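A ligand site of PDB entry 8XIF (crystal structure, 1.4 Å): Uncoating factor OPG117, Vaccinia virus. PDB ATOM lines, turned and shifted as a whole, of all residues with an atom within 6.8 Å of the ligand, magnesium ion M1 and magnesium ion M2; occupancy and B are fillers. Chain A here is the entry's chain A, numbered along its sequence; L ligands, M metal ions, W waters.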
ATOM      1  N   PHE A  53       4.160  16.780  -6.312  1.00  0.00           N
ATOM      2  CA  PHE A  53       4.341  15.937  -5.130  1.00  0.00           C
ATOM      3  C   PHE A  53       3.985  16.745  -3.887  1.00  0.00           C
ATOM      4  O   PHE A  53       4.660  17.716  -3.560  1.00  0.00           O
ATOM      5  CB  PHE A  53       5.790  15.470  -5.067  1.00  0.00           C
ATOM      6  CG  PHE A  53       6.199  14.722  -6.299  1.00  0.00           C
ATOM      7  CD1 PHE A  53       5.930  13.368  -6.429  1.00  0.00           C
ATOM      8  CD2 PHE A  53       6.782  15.387  -7.373  1.00  0.00           C
ATOM      9  CE1 PHE A  53       6.280  12.665  -7.578  1.00  0.00           C
ATOM     10  CE2 PHE A  53       7.116  14.710  -8.541  1.00  0.00           C
ATOM     11  CZ  PHE A  53       6.859  13.341  -8.624  1.00  0.00           C
ATOM     12  N   ASP A  70       0.653   4.258   0.700  1.00  0.00           N
ATOM     13  CA  ASP A  70       1.081   4.087  -0.684  1.00  0.00           C
ATOM     14  C   ASP A  70       1.199   2.590  -0.881  1.00  0.00           C
ATOM     15  O   ASP A  70       2.088   1.973  -0.304  1.00  0.00           O
ATOM     16  CB  ASP A  70       2.444   4.780  -0.832  1.00  0.00           C
ATOM     17  CG  ASP A  70       3.141   4.463  -2.137  1.00  0.00           C
ATOM     18  OD1 ASP A  70       2.457   4.274  -3.172  1.00  0.00           O
ATOM     19  OD2 ASP A  70       4.388   4.426  -2.138  1.00  0.00           O
ATOM     20  N   VAL A  71       0.331   2.006  -1.704  1.00  0.00           N
ATOM     21  CA  VAL A  71       0.274   0.554  -1.882  1.00  0.00           C
ATOM     22  C   VAL A  71       0.825   0.217  -3.269  1.00  0.00           C
ATOM     23  O   VAL A  71       0.290   0.680  -4.290  1.00  0.00           O
ATOM     24  CB  VAL A  71      -1.141   0.001  -1.673  1.00  0.00           C
ATOM     25  CG1 VAL A  71      -1.196  -1.518  -1.994  1.00  0.00           C
ATOM     26  CG2 VAL A  71      -1.614   0.285  -0.219  1.00  0.00           C
ATOM     27  N   ASP A  72       1.875  -0.604  -3.295  1.00  0.00           N
ATOM     28  CA  ASP A  72       2.704  -0.847  -4.480  1.00  0.00           C
ATOM     29  C   ASP A  72       2.738  -2.338  -4.776  1.00  0.00           C
ATOM     30  O   ASP A  72       3.742  -3.002  -4.523  1.00  0.00           O
ATOM     31  CB  ASP A  72       4.149  -0.359  -4.267  1.00  0.00           C
ATOM     32  CG  ASP A  72       4.245   1.156  -4.131  1.00  0.00           C
ATOM     33  OD1 ASP A  72       3.371   1.902  -4.670  1.00  0.00           O
ATOM     34  OD2 ASP A  72       5.180   1.618  -3.428  1.00  0.00           O
ATOM     35  N   SER A 125      -3.917   3.575 -10.078  1.00  0.00           N
ATOM     36  CA  SER A 125      -2.950   3.826 -11.124  1.00  0.00           C
ATOM     37  C   SER A 125      -3.466   3.251 -12.437  1.00  0.00           C
ATOM     38  O   SER A 125      -4.056   2.175 -12.467  1.00  0.00           O
ATOM     39  CB  SER A 125      -1.615   3.147 -10.782  1.00  0.00           C
ATOM     40  OG  SER A 125      -0.758   3.210 -11.926  1.00  0.00           O
ATOM     41  N   ASN A 127      -1.633   2.050 -14.664  1.00  0.00           N
ATOM     42  CA  ASN A 127      -0.778   0.945 -15.103  1.00  0.00           C
ATOM     43  C   ASN A 127      -1.506  -0.364 -14.805  1.00  0.00           C
ATOM     44  O   ASN A 127      -1.573  -0.799 -13.647  1.00  0.00           O
ATOM     45  CB  ASN A 127       0.560   1.008 -14.389  1.00  0.00           C
ATOM     46  CG  ASN A 127       1.549  -0.025 -14.909  1.00  0.00           C
ATOM     47  OD1 ASN A 127       1.165  -1.063 -15.466  1.00  0.00           O
ATOM     48  ND2 ASN A 127       2.844   0.249 -14.713  1.00  0.00           N
ATOM     49  N   LYS A 130       0.042  -3.523 -12.889  1.00  0.00           N
ATOM     50  CA  LYS A 130       0.256  -3.574 -11.448  1.00  0.00           C
ATOM     51  C   LYS A 130      -1.028  -3.159 -10.753  1.00  0.00           C
ATOM     52  O   LYS A 130      -2.028  -2.849 -11.407  1.00  0.00           O
ATOM     53  CB  LYS A 130       1.526  -2.822 -11.047  1.00  0.00           C
ATOM     54  CG  LYS A 130       1.481  -1.368 -11.278  1.00  0.00           C
ATOM     55  CD  LYS A 130       2.875  -0.791 -11.096  1.00  0.00           C
ATOM     56  CE  LYS A 130       2.829   0.715 -10.947  1.00  0.00           C
ATOM     57  NZ  LYS A 130       4.156   1.288 -10.559  1.00  0.00           N
ATOM     58  N   SER A 132      -1.655  -0.563  -8.037  1.00  0.00           N
ATOM     59  CA  SER A 132      -1.021   0.520  -7.320  1.00  0.00           C
ATOM     60  C   SER A 132      -2.089   1.546  -6.972  1.00  0.00           C
ATOM     61  O   SER A 132      -2.912   1.901  -7.824  1.00  0.00           O
ATOM     62  CB  SER A 132       0.019   1.167  -8.220  1.00  0.00           C
ATOM     63  OG  SER A 132       0.278   2.487  -7.760  1.00  0.00           O
ATOM     64  N   PHE A 133      -2.075   2.013  -5.720  1.00  0.00           N
ATOM     65  CA  PHE A 133      -3.039   3.028  -5.334  1.00  0.00           C
ATOM     66  C   PHE A 133      -2.511   3.771  -4.132  1.00  0.00           C
ATOM     67  O   PHE A 133      -1.615   3.313  -3.426  1.00  0.00           O
ATOM     68  CB  PHE A 133      -4.442   2.426  -5.072  1.00  0.00           C
ATOM     69  CG  PHE A 133      -4.503   1.451  -3.913  1.00  0.00           C
ATOM     70  CD1 PHE A 133      -4.691   1.910  -2.621  1.00  0.00           C
ATOM     71  CD2 PHE A 133      -4.441   0.079  -4.134  1.00  0.00           C
ATOM     72  CE1 PHE A 133      -4.772   1.012  -1.524  1.00  0.00           C
ATOM     73  CE2 PHE A 133      -4.537  -0.814  -3.044  1.00  0.00           C
ATOM     74  CZ  PHE A 133      -4.718  -0.350  -1.749  1.00  0.00           C
ATOM     75  N   HIS A 134      -3.057   4.966  -3.929  1.00  0.00           N
ATOM     76  CA  HIS A 134      -2.924   5.712  -2.693  1.00  0.00           C
ATOM     77  C   HIS A 134      -4.250   5.712  -1.955  1.00  0.00           C
ATOM     78  O   HIS A 134      -5.314   5.860  -2.567  1.00  0.00           O
ATOM     79  CB  HIS A 134      -2.477   7.164  -2.925  1.00  0.00           C
ATOM     80  CG  HIS A 134      -1.167   7.277  -3.652  1.00  0.00           C
ATOM     81  ND1 HIS A 134      -0.876   8.341  -4.471  1.00  0.00           N
ATOM     82  CD2 HIS A 134      -0.141   6.394  -3.793  1.00  0.00           C
ATOM     83  CE1 HIS A 134       0.329   8.162  -5.002  1.00  0.00           C
ATOM     84  NE2 HIS A 134       0.785   6.974  -4.613  1.00  0.00           N
ATOM     85  N   SER A 168       1.844  -5.106   0.386  1.00  0.00           N
ATOM     86  CA  SER A 168       2.464  -4.153  -0.523  1.00  0.00           C
ATOM     87  C   SER A 168       2.485  -2.726   0.003  1.00  0.00           C
ATOM     88  O   SER A 168       2.807  -1.816  -0.759  1.00  0.00           O
ATOM     89  CB  SER A 168       1.810  -4.213  -1.912  1.00  0.00           C
ATOM     90  OG  SER A 168       1.878  -5.543  -2.379  1.00  0.00           O
ATOM     91  N   ASP A 170       3.930   0.460   1.310  1.00  0.00           N
ATOM     92  CA  ASP A 170       5.300   0.967   1.207  1.00  0.00           C
ATOM     93  C   ASP A 170       5.522   1.813   2.448  1.00  0.00           C
ATOM     94  O   ASP A 170       5.060   2.958   2.539  1.00  0.00           O
ATOM     95  CB  ASP A 170       5.441   1.790  -0.076  1.00  0.00           C
ATOM     96  CG  ASP A 170       6.828   2.392  -0.236  1.00  0.00           C
ATOM     97  OD1 ASP A 170       7.695   2.183   0.646  1.00  0.00           O
ATOM     98  OD2 ASP A 170       7.083   3.019  -1.303  1.00  0.00           O
ATOM     99  N   ALA A 172       8.264   3.064   3.453  1.00  0.00           N
ATOM    100  CA  ALA A 172       9.341   4.047   3.341  1.00  0.00           C
ATOM    101  C   ALA A 172       8.794   5.467   3.260  1.00  0.00           C
ATOM    102  O   ALA A 172       9.541   6.431   3.487  1.00  0.00           O
ATOM    103  CB  ALA A 172      10.214   3.758   2.129  1.00  0.00           C
ATOM    104  N   VAL A 173       7.494   5.630   2.982  1.00  0.00           N
ATOM    105  CA  VAL A 173       6.933   6.967   2.864  1.00  0.00           C
ATOM    106  C   VAL A 173       6.786   7.646   4.212  1.00  0.00           C
ATOM    107  O   VAL A 173       6.518   8.851   4.243  1.00  0.00           O
ATOM    108  CB  VAL A 173       5.572   6.954   2.132  1.00  0.00           C
ATOM    109  CG1 VAL A 173       5.730   6.287   0.756  1.00  0.00           C
ATOM    110  CG2 VAL A 173       4.471   6.268   2.943  1.00  0.00           C
ATOM    111  N   LEU A 180       3.854  12.757  -1.519  1.00  0.00           N
ATOM    112  CA  LEU A 180       2.881  11.880  -2.145  1.00  0.00           C
ATOM    113  C   LEU A 180       2.498  12.516  -3.469  1.00  0.00           C
ATOM    114  O   LEU A 180       2.042  13.664  -3.500  1.00  0.00           O
ATOM    115  CB  LEU A 180       1.654  11.691  -1.253  1.00  0.00           C
ATOM    116  CG  LEU A 180       0.632  10.661  -1.724  1.00  0.00           C
ATOM    117  CD1 LEU A 180       1.199   9.249  -1.597  1.00  0.00           C
ATOM    118  CD2 LEU A 180      -0.667  10.815  -0.917  1.00  0.00           C
ATOM    119  N   ARG A 181       2.683  11.784  -4.557  1.00  0.00           N
ATOM    120  CA  ARG A 181       2.386  12.342  -5.861  1.00  0.00           C
ATOM    121  C   ARG A 181       0.911  12.734  -5.945  1.00  0.00           C
ATOM    122  O   ARG A 181       0.020  11.978  -5.546  1.00  0.00           O
ATOM    123  CB  ARG A 181       2.738  11.298  -6.915  1.00  0.00           C
ATOM    124  CG  ARG A 181       2.385  11.743  -8.355  1.00  0.00           C
ATOM    125  CD  ARG A 181       3.035  10.864  -9.397  1.00  0.00           C
ATOM    126  NE  ARG A 181       2.697   9.443  -9.319  1.00  0.00           N
ATOM    127  CZ  ARG A 181       2.312   8.712 -10.353  1.00  0.00           C
ATOM    128  NH1 ARG A 181       1.954   9.261 -11.510  1.00  0.00           N
ATOM    129  NH2 ARG A 181       2.323   7.387 -10.246  1.00  0.00           N
ATOM    130  N   VAL A 182       0.649  13.928  -6.486  1.00  0.00           N
ATOM    131  CA  VAL A 182      -0.714  14.439  -6.559  1.00  0.00           C
ATOM    132  C   VAL A 182      -1.504  13.681  -7.629  1.00  0.00           C
ATOM    133  O   VAL A 182      -1.060  13.502  -8.763  1.00  0.00           O
ATOM    134  CB  VAL A 182      -0.730  15.946  -6.858  1.00  0.00           C
ATOM    135  CG1 VAL A 182      -2.168  16.461  -7.011  1.00  0.00           C
ATOM    136  CG2 VAL A 182       0.008  16.689  -5.746  1.00  0.00           C
ATOM    137  N   LYS A 187       4.714  11.020 -12.756  1.00  0.00           N
ATOM    138  CA  LYS A 187       5.862  10.869 -11.867  1.00  0.00           C
ATOM    139  C   LYS A 187       7.110  11.531 -12.416  1.00  0.00           C
ATOM    140  O   LYS A 187       7.912  12.125 -11.670  1.00  0.00           O
ATOM    141  CB  LYS A 187       6.097   9.376 -11.586  1.00  0.00           C
ATOM    142  CG  LYS A 187       7.393   9.013 -10.891  1.00  0.00           C
ATOM    143  CD  LYS A 187       7.387   9.440  -9.444  1.00  0.00           C
ATOM    144  CE  LYS A 187       6.317   8.691  -8.655  1.00  0.00           C
ATOM    145  NZ  LYS A 187       6.087   9.298  -7.321  1.00  0.00           N
ATOM    146  N   THR A 193       1.910   7.283 -17.049  1.00  0.00           N
ATOM    147  CA  THR A 193       0.856   6.765 -16.186  1.00  0.00           C
ATOM    148  C   THR A 193       0.557   7.710 -15.030  1.00  0.00           C
ATOM    149  O   THR A 193       1.452   8.330 -14.459  1.00  0.00           O
ATOM    150  CB  THR A 193       1.206   5.378 -15.635  1.00  0.00           C
ATOM    151  OG1 THR A 193       2.257   5.483 -14.669  1.00  0.00           O
ATOM    152  CG2 THR A 193       1.601   4.455 -16.770  1.00  0.00           C
ATOM    153  N   ILE A 194      -0.726   7.794 -14.702  1.00  0.00           N
ATOM    154  CA  ILE A 194      -1.206   8.624 -13.601  1.00  0.00           C
ATOM    155  C   ILE A 194      -2.087   7.788 -12.708  1.00  0.00           C
ATOM    156  O   ILE A 194      -2.535   6.698 -13.072  1.00  0.00           O
ATOM    157  CB  ILE A 194      -1.993   9.857 -14.077  1.00  0.00           C
ATOM    158  CG1 ILE A 194      -3.272   9.436 -14.855  1.00  0.00           C
ATOM    159  CG2 ILE A 194      -1.103  10.762 -14.917  1.00  0.00           C
ATOM    160  CD1 ILE A 194      -4.282  10.572 -15.095  1.00  0.00           C
ATOM    161  N   HIS A 195      -2.358   8.333 -11.521  1.00  0.00           N
ATOM    162  CA  HIS A 195      -3.458   7.850 -10.692  1.00  0.00           C
ATOM    163  C   HIS A 195      -4.700   8.664 -11.003  1.00  0.00           C
ATOM    164  O   HIS A 195      -4.639   9.890 -11.132  1.00  0.00           O
ATOM    165  CB  HIS A 195      -3.126   8.033  -9.221  1.00  0.00           C
ATOM    166  CG  HIS A 195      -2.093   7.090  -8.725  1.00  0.00           C
ATOM    167  ND1 HIS A 195      -2.212   6.415  -7.530  1.00  0.00           N
ATOM    168  CD2 HIS A 195      -0.910   6.698  -9.265  1.00  0.00           C
ATOM    169  CE1 HIS A 195      -1.166   5.634  -7.370  1.00  0.00           C
ATOM    170  NE2 HIS A 195      -0.355   5.792  -8.387  1.00  0.00           N
HETATM  171  O1  LIG L   1       5.291   6.305  -6.510  1.00  0.00           O
HETATM  172  P1  LIG L   1       3.828   6.521  -6.688  1.00  0.00           P
HETATM  173  O2  LIG L   1       3.453   7.963  -6.933  1.00  0.00           O
HETATM  174  O3  LIG L   1       3.000   5.855  -5.632  1.00  0.00           O
HETATM  175  O4  LIG L   1       3.429   5.789  -8.056  1.00  0.00           O
HETATM  176  P2  LIG L   1       3.275   4.227  -8.419  1.00  0.00           P
HETATM  177  O5  LIG L   1       4.388   3.944  -9.366  1.00  0.00           O
HETATM  178  O6  LIG L   1       3.421   3.456  -7.132  1.00  0.00           O
HETATM  179  O7  LIG L   1       1.911   4.078  -9.026  1.00  0.00           O
HETATM  180 MG    MG M   1       6.063   3.515  -3.066  1.00  0.00          MG
HETATM  181 MG    MG M   2       3.056   3.824  -5.118  1.00  0.00          MG
HETATM  182  O   HOH W   1       0.973   3.402  -5.373  1.00  0.00           O
HETATM  183  O   HOH W   2       6.399   2.887  -7.133  1.00  0.00           O
HETATM  184  O   HOH W   3       1.734   3.547 -11.512  1.00  0.00           O
HETATM  185  O   HOH W   4       7.788   2.812  -4.168  1.00  0.00           O
HETATM  186  O   HOH W   5       7.090   5.365  -3.087  1.00  0.00           O
HETATM  187  O   HOH W   6       3.764   9.173  -4.553  1.00  0.00           O
HETATM  188  O   HOH W   7       5.266   4.038  -4.997  1.00  0.00           O
HETATM  189  O   HOH W   8       3.814   0.693  -7.634  1.00  0.00           O
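NE of Arg 181 lies within salt-bridge range of O2 of the ligand. The side-chain amino group (NZ) of Lys 187 is in salt-bridge range of an oxygen (O2) of the ligand. A ring nitrogen (NE2) of His 195 lies within hydrogen-bond range of an oxygen (O7) of the ligand (2.9 Å). The side-chain hydroxyl of Ser 132 is in hydrogen-bond range of an oxygen (O7) of the ligand, at 2.6 Å. NZ of Lys 130 lies within salt-bridge range of O5 of the ligand (2.9 Å). O3 of the ligand sits close to NE2 of His 134, at 2.7 Å.
The backbone NH of Asp 72 lies within hydrogen-bond range of the backbone carbonyl oxygen of Ser 168 (3.0 Å). The side-chain carboxylate (OD1) of Asp 170 lies within hydrogen-bond range of the backbone NH (N) of Ala 172 (3.0 Å). O of Ser 132 lies within hydrogen-bond range of N of Ser 125 (3.0 Å). The backbone carbonyl oxygen of Thr 193 lies within hydrogen-bond range of the guanidinium group of Arg 181, 3.1 Å away. The side-chain carboxylate (OD1) of Asp 70 sits close to a ring nitrogen (NE2) of His 134. The side-chain hydroxyl of Ser 132 sits at hydrogen-bond distance from a ring nitrogen (NE2) of His 195 (3.4 Å).
Within 4 Å of the ligand: Asp 70, Asp 72, Lys 130, Ser 132, His 134, Arg 181, Lys 187 and His 195. Along chain A the residues within 4 Å of the ligand span positions 70 to 195.
Along chain A the residues within 4 Å of magnesium ion M1 span positions 70 to 170.
Merely in contact with magnesium ion M2: His 134 (3.9 Å).
Magnesium ion M1 is bound by the side-chain carboxylate of Asp 170 (2.1 Å), water W5 (2.1 Å), the side-chain carboxylate of Asp 70 (2.1 Å), the side-chain carboxylate of Asp 72 (2.1 Å), water W7 (2.2 Å) and water W4 (2.2 Å). Magnesium ion M1 has six donor atoms within binding distance.
Magnesium ion M2 is bound by the side-chain carboxylate of Asp 72 (2.0 Å), an oxygen (O6) of the ligand (2.1 Å), the side-chain carboxylate of Asp 70 (2.1 Å), an oxygen (O3) of the ligand (2.1 Å), water W1 (2.1 Å) and water W7 (2.2 Å). Magnesium ion M2 has six donor atoms within binding distance.
Water W1 lies within hydrogen-bond range of the side-chain hydroxyl of Ser 132, the backbone carbonyl oxygen of Val 71 and the backbone carbonyl oxygen of Phe 133. Water W3 lies within hydrogen-bond range of OG of Ser 125 (2.5 Å), O7 of the ligand (2.5 Å) and NZ of Lys 130 (3.4 Å). Water W6 lies within hydrogen-bond range of an oxygen (O2) of the ligand (2.7 Å) and the backbone NH (N) of Arg 181 (2.8 Å).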
